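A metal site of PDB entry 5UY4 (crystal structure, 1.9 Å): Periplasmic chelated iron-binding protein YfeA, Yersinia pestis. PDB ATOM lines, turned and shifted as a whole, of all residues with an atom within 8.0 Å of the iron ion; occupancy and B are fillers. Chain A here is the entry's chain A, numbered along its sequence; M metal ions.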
ATOM      1  N   GLU A  74       2.470 -25.078  -9.520  1.00  0.00           N
ATOM      2  CA  GLU A  74       2.063 -24.134 -10.556  1.00  0.00           C
ATOM      3  C   GLU A  74       3.059 -22.985 -10.624  1.00  0.00           C
ATOM      4  O   GLU A  74       3.355 -22.343  -9.609  1.00  0.00           O
ATOM      5  CB  GLU A  74       0.652 -23.626 -10.234  1.00  0.00           C
ATOM      6  CG  GLU A  74      -0.152 -23.170 -11.423  1.00  0.00           C
ATOM      7  CD  GLU A  74       0.426 -21.904 -12.007  1.00  0.00           C
ATOM      8  OE1 GLU A  74       0.441 -20.873 -11.288  1.00  0.00           O
ATOM      9  OE2 GLU A  74       0.912 -21.955 -13.163  1.00  0.00           O
ATOM     10  N   ILE A  75       3.593 -22.716 -11.823  1.00  0.00           N
ATOM     11  CA  ILE A  75       4.767 -21.855 -11.916  1.00  0.00           C
ATOM     12  C   ILE A  75       4.435 -20.409 -12.291  1.00  0.00           C
ATOM     13  O   ILE A  75       5.203 -19.492 -11.988  1.00  0.00           O
ATOM     14  CB  ILE A  75       5.797 -22.426 -12.913  1.00  0.00           C
ATOM     15  CG1 ILE A  75       5.246 -22.424 -14.340  1.00  0.00           C
ATOM     16  CG2 ILE A  75       6.214 -23.858 -12.501  1.00  0.00           C
ATOM     17  CD1 ILE A  75       6.265 -22.979 -15.360  1.00  0.00           C
ATOM     18  N   HIS A  76       3.315 -20.177 -12.994  1.00  0.00           N
ATOM     19  CA  HIS A  76       3.024 -18.821 -13.460  1.00  0.00           C
ATOM     20  C   HIS A  76       2.767 -17.873 -12.301  1.00  0.00           C
ATOM     21  O   HIS A  76       3.282 -16.756 -12.281  1.00  0.00           O
ATOM     22  CB  HIS A  76       1.809 -18.820 -14.387  1.00  0.00           C
ATOM     23  CG  HIS A  76       1.974 -19.634 -15.640  1.00  0.00           C
ATOM     24  ND1 HIS A  76       2.146 -19.057 -16.872  1.00  0.00           N
ATOM     25  CD2 HIS A  76       1.954 -20.972 -15.839  1.00  0.00           C
ATOM     26  CE1 HIS A  76       2.243 -20.014 -17.786  1.00  0.00           C
ATOM     27  NE2 HIS A  76       2.130 -21.181 -17.184  1.00  0.00           N
ATOM     28  N   LEU A 101       6.812 -15.520 -18.101  1.00  0.00           N
ATOM     29  CA  LEU A 101       6.303 -16.782 -17.553  1.00  0.00           C
ATOM     30  C   LEU A 101       6.100 -16.660 -16.048  1.00  0.00           C
ATOM     31  O   LEU A 101       4.985 -16.877 -15.528  1.00  0.00           O
ATOM     32  CB  LEU A 101       7.292 -17.915 -17.864  1.00  0.00           C
ATOM     33  CG  LEU A 101       6.981 -19.246 -17.152  1.00  0.00           C
ATOM     34  CD1 LEU A 101       5.700 -19.858 -17.682  1.00  0.00           C
ATOM     35  CD2 LEU A 101       8.124 -20.252 -17.294  1.00  0.00           C
ATOM     36  N   ASN A 139       3.287 -15.894 -25.518  1.00  0.00           N
ATOM     37  CA  ASN A 139       3.067 -17.226 -24.951  1.00  0.00           C
ATOM     38  C   ASN A 139       4.399 -17.730 -24.420  1.00  0.00           C
ATOM     39  O   ASN A 139       5.333 -17.903 -25.207  1.00  0.00           O
ATOM     40  CB  ASN A 139       2.528 -18.183 -26.013  1.00  0.00           C
ATOM     41  CG  ASN A 139       2.174 -19.550 -25.461  1.00  0.00           C
ATOM     42  OD1 ASN A 139       2.828 -20.079 -24.545  1.00  0.00           O
ATOM     43  ND2 ASN A 139       1.150 -20.152 -26.032  1.00  0.00           N
ATOM     44  N   PRO A 140       4.544 -17.972 -23.117  1.00  0.00           N
ATOM     45  CA  PRO A 140       5.887 -18.190 -22.554  1.00  0.00           C
ATOM     46  C   PRO A 140       6.412 -19.605 -22.733  1.00  0.00           C
ATOM     47  O   PRO A 140       7.604 -19.846 -22.455  1.00  0.00           O
ATOM     48  CB  PRO A 140       5.677 -17.884 -21.056  1.00  0.00           C
ATOM     49  CG  PRO A 140       4.261 -18.306 -20.814  1.00  0.00           C
ATOM     50  CD  PRO A 140       3.490 -17.962 -22.073  1.00  0.00           C
ATOM     51  N   HIS A 141       5.589 -20.533 -23.231  1.00  0.00           N
ATOM     52  CA  HIS A 141       5.899 -21.954 -23.217  1.00  0.00           C
ATOM     53  C   HIS A 141       6.810 -22.354 -24.388  1.00  0.00           C
ATOM     54  O   HIS A 141       6.548 -23.351 -25.076  1.00  0.00           O
ATOM     55  CB  HIS A 141       4.601 -22.766 -23.263  1.00  0.00           C
ATOM     56  CG  HIS A 141       3.686 -22.493 -22.110  1.00  0.00           C
ATOM     57  ND1 HIS A 141       2.598 -21.640 -22.206  1.00  0.00           N
ATOM     58  CD2 HIS A 141       3.703 -22.946 -20.834  1.00  0.00           C
ATOM     59  CE1 HIS A 141       1.975 -21.593 -21.047  1.00  0.00           C
ATOM     60  NE2 HIS A 141       2.624 -22.367 -20.194  1.00  0.00           N
ATOM     61  N   TRP A 143       9.722 -23.668 -24.582  1.00  0.00           N
ATOM     62  CA  TRP A 143      10.494 -24.903 -24.494  1.00  0.00           C
ATOM     63  C   TRP A 143       9.774 -26.112 -25.073  1.00  0.00           C
ATOM     64  O   TRP A 143      10.396 -27.168 -25.225  1.00  0.00           O
ATOM     65  CB  TRP A 143      10.856 -25.200 -23.033  1.00  0.00           C
ATOM     66  CG  TRP A 143       9.642 -25.380 -22.157  1.00  0.00           C
ATOM     67  CD1 TRP A 143       8.991 -26.561 -21.916  1.00  0.00           C
ATOM     68  CD2 TRP A 143       8.934 -24.377 -21.417  1.00  0.00           C
ATOM     69  NE1 TRP A 143       7.929 -26.352 -21.065  1.00  0.00           N
ATOM     70  CE2 TRP A 143       7.877 -25.032 -20.737  1.00  0.00           C
ATOM     71  CE3 TRP A 143       9.104 -23.001 -21.231  1.00  0.00           C
ATOM     72  CZ2 TRP A 143       6.977 -24.341 -19.933  1.00  0.00           C
ATOM     73  CZ3 TRP A 143       8.205 -22.320 -20.415  1.00  0.00           C
ATOM     74  CH2 TRP A 143       7.151 -22.998 -19.774  1.00  0.00           C
ATOM     75  N   GLU A 207      -4.760 -25.633 -20.356  1.00  0.00           N
ATOM     76  CA  GLU A 207      -3.987 -24.440 -20.695  1.00  0.00           C
ATOM     77  C   GLU A 207      -3.546 -24.498 -22.156  1.00  0.00           C
ATOM     78  O   GLU A 207      -3.199 -25.564 -22.679  1.00  0.00           O
ATOM     79  CB  GLU A 207      -2.761 -24.293 -19.761  1.00  0.00           C
ATOM     80  CG  GLU A 207      -2.086 -22.921 -19.902  1.00  0.00           C
ATOM     81  CD  GLU A 207      -0.739 -22.781 -19.148  1.00  0.00           C
ATOM     82  OE1 GLU A 207      -0.084 -23.787 -18.826  1.00  0.00           O
ATOM     83  OE2 GLU A 207      -0.351 -21.625 -18.909  1.00  0.00           O
ATOM     84  N   GLY A 208      -3.591 -23.357 -22.830  1.00  0.00           N
ATOM     85  CA  GLY A 208      -3.069 -23.250 -24.179  1.00  0.00           C
ATOM     86  C   GLY A 208      -1.552 -23.192 -24.153  1.00  0.00           C
ATOM     87  O   GLY A 208      -0.933 -22.286 -24.715  1.00  0.00           O
ATOM     88  N   ALA A 209      -0.950 -24.193 -23.505  1.00  0.00           N
ATOM     89  CA  ALA A 209       0.485 -24.210 -23.268  1.00  0.00           C
ATOM     90  C   ALA A 209       1.264 -24.907 -24.372  1.00  0.00           C
ATOM     91  O   ALA A 209       2.495 -25.018 -24.264  1.00  0.00           O
ATOM     92  CB  ALA A 209       0.762 -24.890 -21.922  1.00  0.00           C
ATOM     93  N   PHE A 210       0.608 -25.354 -25.436  1.00  0.00           N
ATOM     94  CA  PHE A 210       1.283 -26.240 -26.390  1.00  0.00           C
ATOM     95  C   PHE A 210       1.451 -25.593 -27.758  1.00  0.00           C
ATOM     96  O   PHE A 210       1.780 -26.288 -28.718  1.00  0.00           O
ATOM     97  CB  PHE A 210       0.531 -27.559 -26.481  1.00  0.00           C
ATOM     98  CG  PHE A 210       0.465 -28.268 -25.172  1.00  0.00           C
ATOM     99  CD1 PHE A 210       1.473 -29.138 -24.795  1.00  0.00           C
ATOM    100  CD2 PHE A 210      -0.552 -27.991 -24.263  1.00  0.00           C
ATOM    101  CE1 PHE A 210       1.452 -29.769 -23.561  1.00  0.00           C
ATOM    102  CE2 PHE A 210      -0.596 -28.618 -23.024  1.00  0.00           C
ATOM    103  CZ  PHE A 210       0.413 -29.511 -22.676  1.00  0.00           C
ATOM    104  N   TRP A 225      -8.311 -22.480 -21.430  1.00  0.00           N
ATOM    105  CA  TRP A 225      -7.913 -21.116 -21.095  1.00  0.00           C
ATOM    106  C   TRP A 225      -6.566 -20.819 -21.734  1.00  0.00           C
ATOM    107  O   TRP A 225      -5.755 -21.736 -21.915  1.00  0.00           O
ATOM    108  CB  TRP A 225      -7.853 -20.884 -19.581  1.00  0.00           C
ATOM    109  CG  TRP A 225      -6.995 -21.829 -18.803  1.00  0.00           C
ATOM    110  CD1 TRP A 225      -5.657 -21.680 -18.520  1.00  0.00           C
ATOM    111  CD2 TRP A 225      -7.414 -23.051 -18.177  1.00  0.00           C
ATOM    112  NE1 TRP A 225      -5.227 -22.746 -17.761  1.00  0.00           N
ATOM    113  CE2 TRP A 225      -6.282 -23.596 -17.532  1.00  0.00           C
ATOM    114  CE3 TRP A 225      -8.637 -23.729 -18.091  1.00  0.00           C
ATOM    115  CZ2 TRP A 225      -6.341 -24.802 -16.826  1.00  0.00           C
ATOM    116  CZ3 TRP A 225      -8.690 -24.913 -17.394  1.00  0.00           C
ATOM    117  CH2 TRP A 225      -7.549 -25.437 -16.768  1.00  0.00           C
ATOM    118  N   PRO A 226      -6.317 -19.567 -22.119  1.00  0.00           N
ATOM    119  CA  PRO A 226      -5.123 -19.305 -22.951  1.00  0.00           C
ATOM    120  C   PRO A 226      -3.809 -19.400 -22.195  1.00  0.00           C
ATOM    121  O   PRO A 226      -2.812 -19.879 -22.763  1.00  0.00           O
ATOM    122  CB  PRO A 226      -5.390 -17.899 -23.506  1.00  0.00           C
ATOM    123  CG  PRO A 226      -6.547 -17.346 -22.697  1.00  0.00           C
ATOM    124  CD  PRO A 226      -7.330 -18.496 -22.198  1.00  0.00           C
ATOM    125  N   ILE A 227      -3.774 -18.979 -20.928  1.00  0.00           N
ATOM    126  CA  ILE A 227      -2.590 -19.078 -20.085  1.00  0.00           C
ATOM    127  C   ILE A 227      -3.054 -19.162 -18.634  1.00  0.00           C
ATOM    128  O   ILE A 227      -4.055 -18.534 -18.255  1.00  0.00           O
ATOM    129  CB  ILE A 227      -1.629 -17.880 -20.315  1.00  0.00           C
ATOM    130  CG1 ILE A 227      -0.391 -17.982 -19.420  1.00  0.00           C
ATOM    131  CG2 ILE A 227      -2.355 -16.551 -20.061  1.00  0.00           C
ATOM    132  CD1 ILE A 227       0.726 -16.994 -19.784  1.00  0.00           C
ATOM    133  N   ASN A 228      -2.343 -19.944 -17.819  1.00  0.00           N
ATOM    134  CA  ASN A 228      -2.675 -20.068 -16.391  1.00  0.00           C
ATOM    135  C   ASN A 228      -2.737 -18.692 -15.761  1.00  0.00           C
ATOM    136  O   ASN A 228      -1.850 -17.862 -15.961  1.00  0.00           O
ATOM    137  CB  ASN A 228      -1.636 -20.919 -15.651  1.00  0.00           C
ATOM    138  CG  ASN A 228      -1.724 -22.388 -15.971  1.00  0.00           C
ATOM    139  OD1 ASN A 228      -2.609 -22.845 -16.703  1.00  0.00           O
ATOM    140  ND2 ASN A 228      -0.776 -23.146 -15.437  1.00  0.00           N
ATOM    141  N   ALA A 229      -3.802 -18.460 -14.982  1.00  0.00           N
ATOM    142  CA  ALA A 229      -4.005 -17.215 -14.253  1.00  0.00           C
ATOM    143  C   ALA A 229      -5.348 -17.308 -13.539  1.00  0.00           C
ATOM    144  O   ALA A 229      -6.194 -18.135 -13.892  1.00  0.00           O
ATOM    145  CB  ALA A 229      -4.014 -15.984 -15.189  1.00  0.00           C
ATOM    146  N   GLU A 256      -3.195 -30.963 -17.915  1.00  0.00           N
ATOM    147  CA  GLU A 256      -1.767 -30.846 -17.664  1.00  0.00           C
ATOM    148  C   GLU A 256      -1.448 -31.038 -16.185  1.00  0.00           C
ATOM    149  O   GLU A 256      -2.299 -30.846 -15.311  1.00  0.00           O
ATOM    150  CB  GLU A 256      -1.211 -29.503 -18.134  1.00  0.00           C
ATOM    151  CG  GLU A 256      -1.483 -29.257 -19.606  1.00  0.00           C
ATOM    152  CD  GLU A 256      -2.799 -28.534 -19.815  1.00  0.00           C
ATOM    153  OE1 GLU A 256      -2.995 -27.481 -19.179  1.00  0.00           O
ATOM    154  OE2 GLU A 256      -3.641 -29.035 -20.597  1.00  0.00           O
ATOM    155  N   THR A 258       0.174 -29.592 -13.761  1.00  0.00           N
ATOM    156  CA  THR A 258       0.179 -28.643 -12.652  1.00  0.00           C
ATOM    157  C   THR A 258      -1.175 -27.973 -12.418  1.00  0.00           C
ATOM    158  O   THR A 258      -1.253 -27.070 -11.579  1.00  0.00           O
ATOM    159  CB  THR A 258       1.242 -27.548 -12.827  1.00  0.00           C
ATOM    160  OG1 THR A 258       0.853 -26.663 -13.877  1.00  0.00           O
ATOM    161  CG2 THR A 258       2.607 -28.137 -13.124  1.00  0.00           C
ATOM    162  N   ILE A 259      -2.223 -28.387 -13.133  1.00  0.00           N
ATOM    163  CA  ILE A 259      -3.537 -27.770 -13.031  1.00  0.00           C
ATOM    164  C   ILE A 259      -4.593 -28.880 -12.925  1.00  0.00           C
ATOM    165  O   ILE A 259      -4.309 -30.072 -13.049  1.00  0.00           O
ATOM    166  CB  ILE A 259      -3.838 -26.834 -14.228  1.00  0.00           C
ATOM    167  CG1 ILE A 259      -3.519 -27.502 -15.558  1.00  0.00           C
ATOM    168  CG2 ILE A 259      -3.031 -25.541 -14.115  1.00  0.00           C
ATOM    169  CD1 ILE A 259      -4.682 -28.349 -16.157  1.00  0.00           C
ATOM    170  N   VAL A 281       4.005 -30.033 -19.264  1.00  0.00           N
ATOM    171  CA  VAL A 281       4.545 -28.845 -19.925  1.00  0.00           C
ATOM    172  C   VAL A 281       5.228 -27.918 -18.914  1.00  0.00           C
ATOM    173  O   VAL A 281       6.381 -27.537 -19.096  1.00  0.00           O
ATOM    174  CB  VAL A 281       3.450 -28.097 -20.723  1.00  0.00           C
ATOM    175  CG1 VAL A 281       2.190 -27.911 -19.901  1.00  0.00           C
ATOM    176  CG2 VAL A 281       3.954 -26.742 -21.265  1.00  0.00           C
ATOM    177  N   ASP A 282       4.543 -27.552 -17.830  1.00  0.00           N
ATOM    178  CA  ASP A 282       5.063 -26.559 -16.886  1.00  0.00           C
ATOM    179  C   ASP A 282       5.935 -27.161 -15.791  1.00  0.00           C
ATOM    180  O   ASP A 282       6.544 -26.401 -15.034  1.00  0.00           O
ATOM    181  CB  ASP A 282       3.925 -25.795 -16.203  1.00  0.00           C
ATOM    182  CG  ASP A 282       3.264 -24.812 -17.127  1.00  0.00           C
ATOM    183  OD1 ASP A 282       3.769 -24.638 -18.257  1.00  0.00           O
ATOM    184  OD2 ASP A 282       2.236 -24.220 -16.722  1.00  0.00           O
ATOM    185  N   SER A 283       5.997 -28.481 -15.668  1.00  0.00           N
ATOM    186  CA  SER A 283       6.809 -29.062 -14.616  1.00  0.00           C
ATOM    187  C   SER A 283       7.216 -30.484 -15.002  1.00  0.00           C
ATOM    188  O   SER A 283       6.487 -31.197 -15.693  1.00  0.00           O
ATOM    189  CB  SER A 283       6.069 -29.069 -13.264  1.00  0.00           C
ATOM    190  OG  SER A 283       6.848 -29.693 -12.258  1.00  0.00           O
HETATM  191 FE    FE M   1       1.780 -22.871 -18.303  1.00  0.00          FE
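The side-chain carboxylate (OE2) of Glu 74 lies within hydrogen-bond range of the backbone NH (N) of His 76, at 3.0 Å. The side-chain carboxylate (OD2) of Asp 282 sits close to the side-chain amide nitrogen (ND2) of Asn 228 (3.4 Å). A ring nitrogen (ND1) of His 141 sits at hydrogen-bond distance from the side-chain amide oxygen (OD1) of Asn 139 (2.8 Å). The side-chain carboxylate (OE2) of Glu 207 lies close to the backbone NH (N) of Asn 228 (2.8 Å). The backbone NH (N) of Glu 207 is in hydrogen-bond range of the side-chain carboxylate (OE1) of Glu 256, 2.8 Å away. The side-chain carboxylate (OE2) of Glu 74 is in hydrogen-bond range of the side-chain amide nitrogen (ND2) of Asn 228, at 3.1 Å. The side-chain amide oxygen of Asn 228 sits at hydrogen-bond distance from the indole nitrogen of Trp 225.
ND2 of Asn 228 touches the iron ion, 3.9 Å away. Along chain A the residues within 4 Å of the iron ion span positions 76 to 282.
The iron ion is bound by a ring nitrogen (NE2) of His 76, the side-chain carboxylate (OD2) of Asp 282, a ring nitrogen (NE2) of His 141, the side-chain carboxylate (OE1) of Glu 207 and the side-chain carboxylate (OE2) of Glu 207. The iron ion has five donor atoms within binding distance. Slightly farther from the iron ion lies the side-chain carboxylate (OD1) of Asp 282 (2.7 Å).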
